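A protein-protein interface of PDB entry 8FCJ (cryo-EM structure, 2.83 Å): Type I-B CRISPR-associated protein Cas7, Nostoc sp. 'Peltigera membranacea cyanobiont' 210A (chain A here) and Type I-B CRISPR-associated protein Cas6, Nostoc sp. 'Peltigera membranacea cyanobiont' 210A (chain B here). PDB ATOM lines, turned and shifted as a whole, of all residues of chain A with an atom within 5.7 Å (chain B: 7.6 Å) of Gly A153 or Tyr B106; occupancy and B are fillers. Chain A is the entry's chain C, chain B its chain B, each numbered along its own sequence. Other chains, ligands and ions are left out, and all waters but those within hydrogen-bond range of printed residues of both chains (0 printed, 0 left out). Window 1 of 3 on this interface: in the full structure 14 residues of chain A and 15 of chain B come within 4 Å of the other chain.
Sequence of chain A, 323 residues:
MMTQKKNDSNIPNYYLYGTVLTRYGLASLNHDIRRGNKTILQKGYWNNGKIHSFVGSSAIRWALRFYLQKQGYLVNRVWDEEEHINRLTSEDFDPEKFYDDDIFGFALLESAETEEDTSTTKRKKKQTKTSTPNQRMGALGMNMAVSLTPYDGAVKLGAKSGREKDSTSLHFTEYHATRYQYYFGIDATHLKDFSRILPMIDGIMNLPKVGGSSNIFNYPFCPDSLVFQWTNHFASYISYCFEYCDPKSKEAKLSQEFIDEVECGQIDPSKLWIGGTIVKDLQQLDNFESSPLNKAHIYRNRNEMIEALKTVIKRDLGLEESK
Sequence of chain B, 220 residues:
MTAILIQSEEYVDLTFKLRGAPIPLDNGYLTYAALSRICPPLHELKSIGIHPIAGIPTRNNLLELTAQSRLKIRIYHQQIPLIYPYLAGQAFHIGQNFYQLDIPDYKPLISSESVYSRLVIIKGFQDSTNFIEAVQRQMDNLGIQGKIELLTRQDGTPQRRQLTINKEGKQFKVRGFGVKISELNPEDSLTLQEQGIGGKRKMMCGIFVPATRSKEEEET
NZ of Lys A38 lies within hydrogen-bond range of O of Tyr B106 (2.7 Å).
O of Gly A153 sits at hydrogen-bond distance from OH of Tyr B106 (3.1 Å).
The side-chain carboxylate of Glu A174 lies close to the side-chain hydroxyl of Tyr B106 (3.3 Å).
Gly A153 touches just these residues of chain B: Ile B80, Tyr B84 and Tyr B106.
Tyr B106 touches five residues of chain A.
Of the printed residues of chain B, Asp A152 touches Pro B81 (3.2 Å) and Tyr B84 (3.2 Å).
Printed residues of chain A within 4 Å of Val B12: Phe A172.
Printed residues of chain A within 4 Å of Asp B105: Lys A38 (3.2 Å).
The nearest residue of chain B that does not touch Gly A153 is Pro B81 (4.7 Å).
The nearest residue of chain A that does not touch Tyr B106 is Val A155 (4.3 Å).
O of Val B12 is in hydrogen-bond range of N of Ile B75.
N of Thr B15 is in hydrogen-bond range of O of Asp B105, 3.0 Å away.
NZ of Lys B107 is in salt-bridge range of OD2 of Asp B105, 3.6 Å away.
The side-chain hydroxyl of Tyr A151 sits at hydrogen-bond distance from the backbone carbonyl oxygen of Ala A154 (2.9 Å).
OH of Tyr A151 lies close to OE2 of Glu A174, 3.4 Å away.
The side-chain carboxylate of Asp A152 sits close to the backbone NH of Ala A154 (3.3 Å).
Hydrophobic or aromatic side chains of chain A that line the printed part of chain B: Tyr A151, Ala A154 and Phe A172.
Along chain A the printed residues that touch a printed residue of chain B span positions 38 to 174.
Among the printed residues, 13 pairs touch across the chains.
Among the printed residues, no Asp or Glu carboxylate lies within 4 Å of a Lys or Arg side-chain nitrogen of the other chain.
Among the printed residues, pairs that only touch across the chains: Asp A152 with Tyr B84, Asp A152 with Pro B81, Lys A38 with Asp B105, Gly A153 with Ile B80, Phe A172 with Tyr B106, Tyr A151 with Tyr B84, Gly A153 with Tyr B84, Phe A172 with Val B12, Tyr A151 with Tyr B106 and Ala A154 with Pro B81.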
ATOM      1  N   LYS A  38      -3.729  -8.939  23.442  1.00  0.00           N
ATOM      2  CA  LYS A  38      -5.096  -8.513  23.198  1.00  0.00           C
ATOM      3  C   LYS A  38      -5.873  -8.379  24.501  1.00  0.00           C
ATOM      4  O   LYS A  38      -5.671  -9.137  25.453  1.00  0.00           O
ATOM      5  CB  LYS A  38      -5.803  -9.505  22.277  1.00  0.00           C
ATOM      6  CG  LYS A  38      -5.130 -10.861  22.213  1.00  0.00           C
ATOM      7  CD  LYS A  38      -5.739 -11.734  21.134  1.00  0.00           C
ATOM      8  CE  LYS A  38      -4.895 -12.974  20.908  1.00  0.00           C
ATOM      9  NZ  LYS A  38      -3.676 -12.681  20.107  1.00  0.00           N
ATOM     10  N   ILE A  40      -9.541  -8.721  25.048  1.00  0.00           N
ATOM     11  CA  ILE A  40     -10.768  -9.139  24.384  1.00  0.00           C
ATOM     12  C   ILE A  40     -11.947  -9.040  25.343  1.00  0.00           C
ATOM     13  O   ILE A  40     -11.785  -9.098  26.568  1.00  0.00           O
ATOM     14  CB  ILE A  40     -10.599 -10.547  23.763  1.00  0.00           C
ATOM     15  CG1 ILE A  40     -10.192 -11.666  24.756  1.00  0.00           C
ATOM     16  CG2 ILE A  40      -9.617 -10.490  22.596  1.00  0.00           C
ATOM     17  CD1 ILE A  40     -11.074 -11.957  25.957  1.00  0.00           C
ATOM     18  N   TYR A 151     -22.355  -9.260  18.711  1.00  0.00           N
ATOM     19  CA  TYR A 151     -21.022  -8.689  18.576  1.00  0.00           C
ATOM     20  C   TYR A 151     -20.543  -8.810  17.136  1.00  0.00           C
ATOM     21  O   TYR A 151     -20.557  -9.898  16.554  1.00  0.00           O
ATOM     22  CB  TYR A 151     -20.054  -9.391  19.524  1.00  0.00           C
ATOM     23  CG  TYR A 151     -18.631  -8.896  19.440  1.00  0.00           C
ATOM     24  CD1 TYR A 151     -18.351  -7.543  19.331  1.00  0.00           C
ATOM     25  CD2 TYR A 151     -17.566  -9.782  19.480  1.00  0.00           C
ATOM     26  CE1 TYR A 151     -17.053  -7.088  19.259  1.00  0.00           C
ATOM     27  CE2 TYR A 151     -16.265  -9.337  19.409  1.00  0.00           C
ATOM     28  CZ  TYR A 151     -16.015  -7.989  19.298  1.00  0.00           C
ATOM     29  OH  TYR A 151     -14.719  -7.540  19.225  1.00  0.00           O
ATOM     30  N   ASP A 152     -20.117  -7.685  16.562  1.00  0.00           N
ATOM     31  CA  ASP A 152     -19.692  -7.651  15.170  1.00  0.00           C
ATOM     32  C   ASP A 152     -18.221  -7.987  14.984  1.00  0.00           C
ATOM     33  O   ASP A 152     -17.752  -8.019  13.845  1.00  0.00           O
ATOM     34  CB  ASP A 152     -19.976  -6.275  14.565  1.00  0.00           C
ATOM     35  CG  ASP A 152     -19.620  -5.142  15.506  1.00  0.00           C
ATOM     36  OD1 ASP A 152     -18.791  -5.357  16.413  1.00  0.00           O
ATOM     37  OD2 ASP A 152     -20.167  -4.032  15.335  1.00  0.00           O
ATOM     38  N   GLY A 153     -17.482  -8.225  16.063  1.00  0.00           N
ATOM     39  CA  GLY A 153     -16.081  -8.561  15.943  1.00  0.00           C
ATOM     40  C   GLY A 153     -15.160  -7.396  15.675  1.00  0.00           C
ATOM     41  O   GLY A 153     -13.993  -7.618  15.336  1.00  0.00           O
ATOM     42  N   ALA A 154     -15.645  -6.164  15.808  1.00  0.00           N
ATOM     43  CA  ALA A 154     -14.803  -5.000  15.570  1.00  0.00           C
ATOM     44  C   ALA A 154     -13.656  -4.957  16.568  1.00  0.00           C
ATOM     45  O   ALA A 154     -13.833  -5.234  17.758  1.00  0.00           O
ATOM     46  CB  ALA A 154     -15.632  -3.720  15.663  1.00  0.00           C
ATOM     47  N   VAL A 155     -12.472  -4.610  16.076  1.00  0.00           N
ATOM     48  CA  VAL A 155     -11.271  -4.533  16.896  1.00  0.00           C
ATOM     49  C   VAL A 155     -10.581  -3.209  16.607  1.00  0.00           C
ATOM     50  O   VAL A 155     -10.753  -2.615  15.539  1.00  0.00           O
ATOM     51  CB  VAL A 155     -10.325  -5.728  16.634  1.00  0.00           C
ATOM     52  CG1 VAL A 155      -9.607  -5.567  15.306  1.00  0.00           C
ATOM     53  CG2 VAL A 155      -9.337  -5.902  17.778  1.00  0.00           C
ATOM     54  N   PHE A 172      -4.164  -5.421  20.546  1.00  0.00           N
ATOM     55  CA  PHE A 172      -5.542  -5.421  20.079  1.00  0.00           C
ATOM     56  C   PHE A 172      -6.487  -5.165  21.243  1.00  0.00           C
ATOM     57  O   PHE A 172      -6.369  -5.798  22.296  1.00  0.00           O
ATOM     58  CB  PHE A 172      -5.883  -6.754  19.413  1.00  0.00           C
ATOM     59  CG  PHE A 172      -5.150  -6.999  18.122  1.00  0.00           C
ATOM     60  CD1 PHE A 172      -4.286  -6.050  17.599  1.00  0.00           C
ATOM     61  CD2 PHE A 172      -5.310  -8.191  17.443  1.00  0.00           C
ATOM     62  CE1 PHE A 172      -3.612  -6.283  16.418  1.00  0.00           C
ATOM     63  CE2 PHE A 172      -4.638  -8.429  16.263  1.00  0.00           C
ATOM     64  CZ  PHE A 172      -3.787  -7.474  15.750  1.00  0.00           C
ATOM     65  N   GLU A 174     -10.796  -4.727  21.979  1.00  0.00           N
ATOM     66  CA  GLU A 174     -12.104  -4.947  21.382  1.00  0.00           C
ATOM     67  C   GLU A 174     -13.103  -3.922  21.892  1.00  0.00           C
ATOM     68  O   GLU A 174     -13.168  -3.634  23.091  1.00  0.00           O
ATOM     69  CB  GLU A 174     -12.612  -6.353  21.693  1.00  0.00           C
ATOM     70  CG  GLU A 174     -11.948  -7.458  20.903  1.00  0.00           C
ATOM     71  CD  GLU A 174     -12.544  -8.814  21.215  1.00  0.00           C
ATOM     72  OE1 GLU A 174     -13.138  -8.967  22.301  1.00  0.00           O
ATOM     73  OE2 GLU A 174     -12.427  -9.727  20.374  1.00  0.00           O
ATOM     74  N   TYR A 175     -13.886  -3.370  20.973  1.00  0.00           N
ATOM     75  CA  TYR A 175     -14.946  -2.439  21.314  1.00  0.00           C
ATOM     76  C   TYR A 175     -16.232  -2.876  20.633  1.00  0.00           C
ATOM     77  O   TYR A 175     -16.220  -3.367  19.502  1.00  0.00           O
ATOM     78  CB  TYR A 175     -14.590  -1.003  20.909  1.00  0.00           C
ATOM     79  CG  TYR A 175     -14.604  -0.757  19.421  1.00  0.00           C
ATOM     80  CD1 TYR A 175     -13.505  -1.071  18.637  1.00  0.00           C
ATOM     81  CD2 TYR A 175     -15.712  -0.199  18.801  1.00  0.00           C
ATOM     82  CE1 TYR A 175     -13.513  -0.845  17.277  1.00  0.00           C
ATOM     83  CE2 TYR A 175     -15.728   0.030  17.443  1.00  0.00           C
ATOM     84  CZ  TYR A 175     -14.627  -0.294  16.686  1.00  0.00           C
ATOM     85  OH  TYR A 175     -14.641  -0.065  15.331  1.00  0.00           O
ATOM     86  N   VAL B  12      -4.807  -8.625  10.047  1.00  0.00           N
ATOM     87  CA  VAL B  12      -4.802  -9.592  11.134  1.00  0.00           C
ATOM     88  C   VAL B  12      -5.117 -10.965  10.557  1.00  0.00           C
ATOM     89  O   VAL B  12      -5.409 -11.115   9.371  1.00  0.00           O
ATOM     90  CB  VAL B  12      -5.806  -9.234  12.248  1.00  0.00           C
ATOM     91  CG1 VAL B  12      -5.572  -7.821  12.751  1.00  0.00           C
ATOM     92  CG2 VAL B  12      -7.228  -9.396  11.747  1.00  0.00           C
ATOM     93  N   ASP B  13      -5.054 -11.975  11.420  1.00  0.00           N
ATOM     94  CA  ASP B  13      -5.370 -13.353  11.053  1.00  0.00           C
ATOM     95  C   ASP B  13      -6.495 -13.839  11.961  1.00  0.00           C
ATOM     96  O   ASP B  13      -6.273 -14.120  13.142  1.00  0.00           O
ATOM     97  CB  ASP B  13      -4.139 -14.246  11.163  1.00  0.00           C
ATOM     98  CG  ASP B  13      -3.301 -14.235   9.904  1.00  0.00           C
ATOM     99  OD1 ASP B  13      -3.230 -13.176   9.247  1.00  0.00           O
ATOM    100  OD2 ASP B  13      -2.710 -15.282   9.569  1.00  0.00           O
ATOM    101  N   LEU B  14      -7.700 -13.934  11.407  1.00  0.00           N
ATOM    102  CA  LEU B  14      -8.857 -14.424  12.148  1.00  0.00           C
ATOM    103  C   LEU B  14      -8.817 -15.946  12.152  1.00  0.00           C
ATOM    104  O   LEU B  14      -9.027 -16.582  11.114  1.00  0.00           O
ATOM    105  CB  LEU B  14     -10.144 -13.903  11.518  1.00  0.00           C
ATOM    106  CG  LEU B  14     -11.331 -13.652  12.445  1.00  0.00           C
ATOM    107  CD1 LEU B  14     -10.970 -12.619  13.490  1.00  0.00           C
ATOM    108  CD2 LEU B  14     -12.534 -13.197  11.642  1.00  0.00           C
ATOM    109  N   THR B  15      -8.552 -16.537  13.313  1.00  0.00           N
ATOM    110  CA  THR B  15      -8.365 -17.978  13.439  1.00  0.00           C
ATOM    111  C   THR B  15      -9.556 -18.585  14.166  1.00  0.00           C
ATOM    112  O   THR B  15      -9.825 -18.240  15.320  1.00  0.00           O
ATOM    113  CB  THR B  15      -7.072 -18.298  14.189  1.00  0.00           C
ATOM    114  OG1 THR B  15      -7.315 -18.248  15.600  1.00  0.00           O
ATOM    115  CG2 THR B  15      -5.991 -17.292  13.837  1.00  0.00           C
ATOM    116  N   ILE B  75      -7.397 -10.922   6.718  1.00  0.00           N
ATOM    117  CA  ILE B  75      -8.390  -9.938   6.307  1.00  0.00           C
ATOM    118  C   ILE B  75      -8.002  -8.576   6.864  1.00  0.00           C
ATOM    119  O   ILE B  75      -7.381  -8.471   7.924  1.00  0.00           O
ATOM    120  CB  ILE B  75      -9.807 -10.356   6.771  1.00  0.00           C
ATOM    121  CG1 ILE B  75     -10.874  -9.393   6.247  1.00  0.00           C
ATOM    122  CG2 ILE B  75      -9.864 -10.457   8.286  1.00  0.00           C
ATOM    123  CD1 ILE B  75     -10.848  -9.202   4.751  1.00  0.00           C
ATOM    124  N   HIS B  77      -8.396  -5.452   8.941  1.00  0.00           N
ATOM    125  CA  HIS B  77      -8.999  -5.437  10.269  1.00  0.00           C
ATOM    126  C   HIS B  77     -10.275  -4.606  10.330  1.00  0.00           C
ATOM    127  O   HIS B  77     -11.090  -4.818  11.233  1.00  0.00           O
ATOM    128  CB  HIS B  77      -7.993  -4.933  11.305  1.00  0.00           C
ATOM    129  CG  HIS B  77      -7.852  -3.444  11.341  1.00  0.00           C
ATOM    130  ND1 HIS B  77      -7.843  -2.727  12.518  1.00  0.00           N
ATOM    131  CD2 HIS B  77      -7.708  -2.536  10.347  1.00  0.00           C
ATOM    132  CE1 HIS B  77      -7.703  -1.441  12.247  1.00  0.00           C
ATOM    133  NE2 HIS B  77      -7.620  -1.299  10.937  1.00  0.00           N
ATOM    134  N   GLN B  79     -12.497  -4.733   7.884  1.00  0.00           N
ATOM    135  CA  GLN B  79     -13.492  -5.522   7.174  1.00  0.00           C
ATOM    136  C   GLN B  79     -13.959  -6.737   7.960  1.00  0.00           C
ATOM    137  O   GLN B  79     -14.777  -7.509   7.450  1.00  0.00           O
ATOM    138  CB  GLN B  79     -12.944  -5.968   5.815  1.00  0.00           C
ATOM    139  CG  GLN B  79     -12.531  -4.823   4.909  1.00  0.00           C
ATOM    140  CD  GLN B  79     -12.262  -5.279   3.490  1.00  0.00           C
ATOM    141  OE1 GLN B  79     -12.967  -6.136   2.958  1.00  0.00           O
ATOM    142  NE2 GLN B  79     -11.235  -4.710   2.871  1.00  0.00           N
ATOM    143  N   ILE B  80     -13.454  -6.931   9.179  1.00  0.00           N
ATOM    144  CA  ILE B  80     -13.932  -8.036  10.010  1.00  0.00           C
ATOM    145  C   ILE B  80     -15.429  -7.943  10.286  1.00  0.00           C
ATOM    146  O   ILE B  80     -16.127  -8.956  10.117  1.00  0.00           O
ATOM    147  CB  ILE B  80     -13.097  -8.129  11.301  1.00  0.00           C
ATOM    148  CG1 ILE B  80     -11.668  -8.559  10.978  1.00  0.00           C
ATOM    149  CG2 ILE B  80     -13.732  -9.100  12.276  1.00  0.00           C
ATOM    150  CD1 ILE B  80     -10.854  -8.924  12.196  1.00  0.00           C
ATOM    151  N   PRO B  81     -15.999  -6.778  10.676  1.00  0.00           N
ATOM    152  CA  PRO B  81     -17.442  -6.732  10.957  1.00  0.00           C
ATOM    153  C   PRO B  81     -18.331  -7.110   9.781  1.00  0.00           C
ATOM    154  O   PRO B  81     -19.554  -7.191   9.932  1.00  0.00           O
ATOM    155  CB  PRO B  81     -17.667  -5.272  11.367  1.00  0.00           C
ATOM    156  CG  PRO B  81     -16.367  -4.839  11.906  1.00  0.00           C
ATOM    157  CD  PRO B  81     -15.350  -5.504  11.036  1.00  0.00           C
ATOM    158  N   LEU B  82     -17.742  -7.341   8.608  1.00  0.00           N
ATOM    159  CA  LEU B  82     -18.510  -7.786   7.455  1.00  0.00           C
ATOM    160  C   LEU B  82     -18.702  -9.296   7.412  1.00  0.00           C
ATOM    161  O   LEU B  82     -19.668  -9.764   6.801  1.00  0.00           O
ATOM    162  CB  LEU B  82     -17.833  -7.327   6.160  1.00  0.00           C
ATOM    163  CG  LEU B  82     -17.419  -5.858   6.105  1.00  0.00           C
ATOM    164  CD1 LEU B  82     -16.540  -5.597   4.895  1.00  0.00           C
ATOM    165  CD2 LEU B  82     -18.643  -4.960   6.082  1.00  0.00           C
ATOM    166  N   TYR B  84     -17.626 -11.400  10.447  1.00  0.00           N
ATOM    167  CA  TYR B  84     -17.616 -11.973  11.792  1.00  0.00           C
ATOM    168  C   TYR B  84     -18.973 -12.512  12.224  1.00  0.00           C
ATOM    169  O   TYR B  84     -19.029 -13.664  12.690  1.00  0.00           O
ATOM    170  CB  TYR B  84     -17.079 -10.932  12.781  1.00  0.00           C
ATOM    171  CG  TYR B  84     -16.854 -11.444  14.187  1.00  0.00           C
ATOM    172  CD1 TYR B  84     -17.907 -11.570  15.083  1.00  0.00           C
ATOM    173  CD2 TYR B  84     -15.583 -11.785  14.622  1.00  0.00           C
ATOM    174  CE1 TYR B  84     -17.700 -12.028  16.366  1.00  0.00           C
ATOM    175  CE2 TYR B  84     -15.369 -12.240  15.905  1.00  0.00           C
ATOM    176  CZ  TYR B  84     -16.430 -12.364  16.772  1.00  0.00           C
ATOM    177  OH  TYR B  84     -16.216 -12.822  18.049  1.00  0.00           O
ATOM    178  N   PRO B  85     -20.084 -11.772  12.120  1.00  0.00           N
ATOM    179  CA  PRO B  85     -21.367 -12.332  12.579  1.00  0.00           C
ATOM    180  C   PRO B  85     -21.800 -13.570  11.818  1.00  0.00           C
ATOM    181  O   PRO B  85     -22.542 -14.389  12.373  1.00  0.00           O
ATOM    182  CB  PRO B  85     -22.354 -11.175  12.375  1.00  0.00           C
ATOM    183  CG  PRO B  85     -21.717 -10.301  11.367  1.00  0.00           C
ATOM    184  CD  PRO B  85     -20.250 -10.398  11.613  1.00  0.00           C
ATOM    185  N   ALA B  88     -18.493 -16.438  13.210  1.00  0.00           N
ATOM    186  CA  ALA B  88     -18.204 -16.690  14.618  1.00  0.00           C
ATOM    187  C   ALA B  88     -19.384 -17.397  15.268  1.00  0.00           C
ATOM    188  O   ALA B  88     -20.470 -16.822  15.396  1.00  0.00           O
ATOM    189  CB  ALA B  88     -17.894 -15.380  15.334  1.00  0.00           C
ATOM    190  N   ILE B 103     -15.689 -18.864  18.749  1.00  0.00           N
ATOM    191  CA  ILE B 103     -15.252 -17.471  18.763  1.00  0.00           C
ATOM    192  C   ILE B 103     -13.810 -17.406  18.279  1.00  0.00           C
ATOM    193  O   ILE B 103     -12.930 -18.060  18.858  1.00  0.00           O
ATOM    194  CB  ILE B 103     -15.387 -16.856  20.165  1.00  0.00           C
ATOM    195  CG1 ILE B 103     -16.840 -16.896  20.631  1.00  0.00           C
ATOM    196  CG2 ILE B 103     -14.866 -15.432  20.168  1.00  0.00           C
ATOM    197  CD1 ILE B 103     -17.051 -17.686  21.901  1.00  0.00           C
ATOM    198  N   PRO B 104     -13.520 -16.639  17.236  1.00  0.00           N
ATOM    199  CA  PRO B 104     -12.159 -16.600  16.700  1.00  0.00           C
ATOM    200  C   PRO B 104     -11.221 -15.784  17.574  1.00  0.00           C
ATOM    201  O   PRO B 104     -11.635 -14.994  18.423  1.00  0.00           O
ATOM    202  CB  PRO B 104     -12.341 -15.940  15.331  1.00  0.00           C
ATOM    203  CG  PRO B 104     -13.524 -15.077  15.505  1.00  0.00           C
ATOM    204  CD  PRO B 104     -14.441 -15.801  16.453  1.00  0.00           C
ATOM    205  N   ASP B 105      -9.931 -15.999  17.345  1.00  0.00           N
ATOM    206  CA  ASP B 105      -8.875 -15.237  17.988  1.00  0.00           C
ATOM    207  C   ASP B 105      -8.086 -14.488  16.923  1.00  0.00           C
ATOM    208  O   ASP B 105      -7.965 -14.945  15.783  1.00  0.00           O
ATOM    209  CB  ASP B 105      -7.942 -16.145  18.794  1.00  0.00           C
ATOM    210  CG  ASP B 105      -7.380 -15.459  20.021  1.00  0.00           C
ATOM    211  OD1 ASP B 105      -7.738 -14.286  20.260  1.00  0.00           O
ATOM    212  OD2 ASP B 105      -6.581 -16.088  20.746  1.00  0.00           O
ATOM    213  N   TYR B 106      -7.555 -13.332  17.302  1.00  0.00           N
ATOM    214  CA  TYR B 106      -6.804 -12.485  16.387  1.00  0.00           C
ATOM    215  C   TYR B 106      -5.314 -12.741  16.556  1.00  0.00           C
ATOM    216  O   TYR B 106      -4.810 -12.779  17.682  1.00  0.00           O
ATOM    217  CB  TYR B 106      -7.111 -11.006  16.625  1.00  0.00           C
ATOM    218  CG  TYR B 106      -8.579 -10.683  16.760  1.00  0.00           C
ATOM    219  CD1 TYR B 106      -9.229 -10.806  17.978  1.00  0.00           C
ATOM    220  CD2 TYR B 106      -9.314 -10.242  15.668  1.00  0.00           C
ATOM    221  CE1 TYR B 106     -10.567 -10.510  18.104  1.00  0.00           C
ATOM    222  CE2 TYR B 106     -10.655  -9.942  15.786  1.00  0.00           C
ATOM    223  CZ  TYR B 106     -11.276 -10.079  17.006  1.00  0.00           C
ATOM    224  OH  TYR B 106     -12.613  -9.781  17.129  1.00  0.00           O
ATOM    225  N   LYS B 107      -4.618 -12.919  15.437  1.00  0.00           N
ATOM    226  CA  LYS B 107      -3.181 -13.099  15.434  1.00  0.00           C
ATOM    227  C   LYS B 107      -2.534 -12.016  14.583  1.00  0.00           C
ATOM    228  O   LYS B 107      -2.902 -11.853  13.412  1.00  0.00           O
ATOM    229  CB  LYS B 107      -2.800 -14.486  14.897  1.00  0.00           C
ATOM    230  CG  LYS B 107      -3.213 -15.626  15.808  1.00  0.00           C
ATOM    231  CD  LYS B 107      -2.697 -15.404  17.218  1.00  0.00           C
ATOM    232  CE  LYS B 107      -3.273 -16.424  18.183  1.00  0.00           C
ATOM    233  NZ  LYS B 107      -4.659 -16.821  17.818  1.00  0.00           N
ATOM    234  N   PRO B 108      -1.588 -11.257  15.126  1.00  0.00           N
ATOM    235  CA  PRO B 108      -0.949 -10.202  14.336  1.00  0.00           C
ATOM    236  C   PRO B 108      -0.074 -10.782  13.238  1.00  0.00           C
ATOM    237  O   PRO B 108       0.398 -11.918  13.307  1.00  0.00           O
ATOM    238  CB  PRO B 108      -0.114  -9.440  15.370  1.00  0.00           C
ATOM    239  CG  PRO B 108       0.174 -10.446  16.428  1.00  0.00           C
ATOM    240  CD  PRO B 108      -0.996 -11.389  16.467  1.00  0.00           C
ATOM    241  N   LEU B 109       0.137  -9.972  12.204  1.00  0.00           N
ATOM    242  CA  LEU B 109       0.956 -10.364  11.064  1.00  0.00           C
ATOM    243  C   LEU B 109       2.406  -9.998  11.361  1.00  0.00           C
ATOM    244  O   LEU B 109       2.781  -8.823  11.314  1.00  0.00           O
ATOM    245  CB  LEU B 109       0.459  -9.687   9.790  1.00  0.00           C
ATOM    246  CG  LEU B 109       0.376 -10.579   8.553  1.00  0.00           C
ATOM    247  CD1 LEU B 109      -0.240 -11.918   8.911  1.00  0.00           C
ATOM    248  CD2 LEU B 109      -0.430  -9.899   7.465  1.00  0.00           C
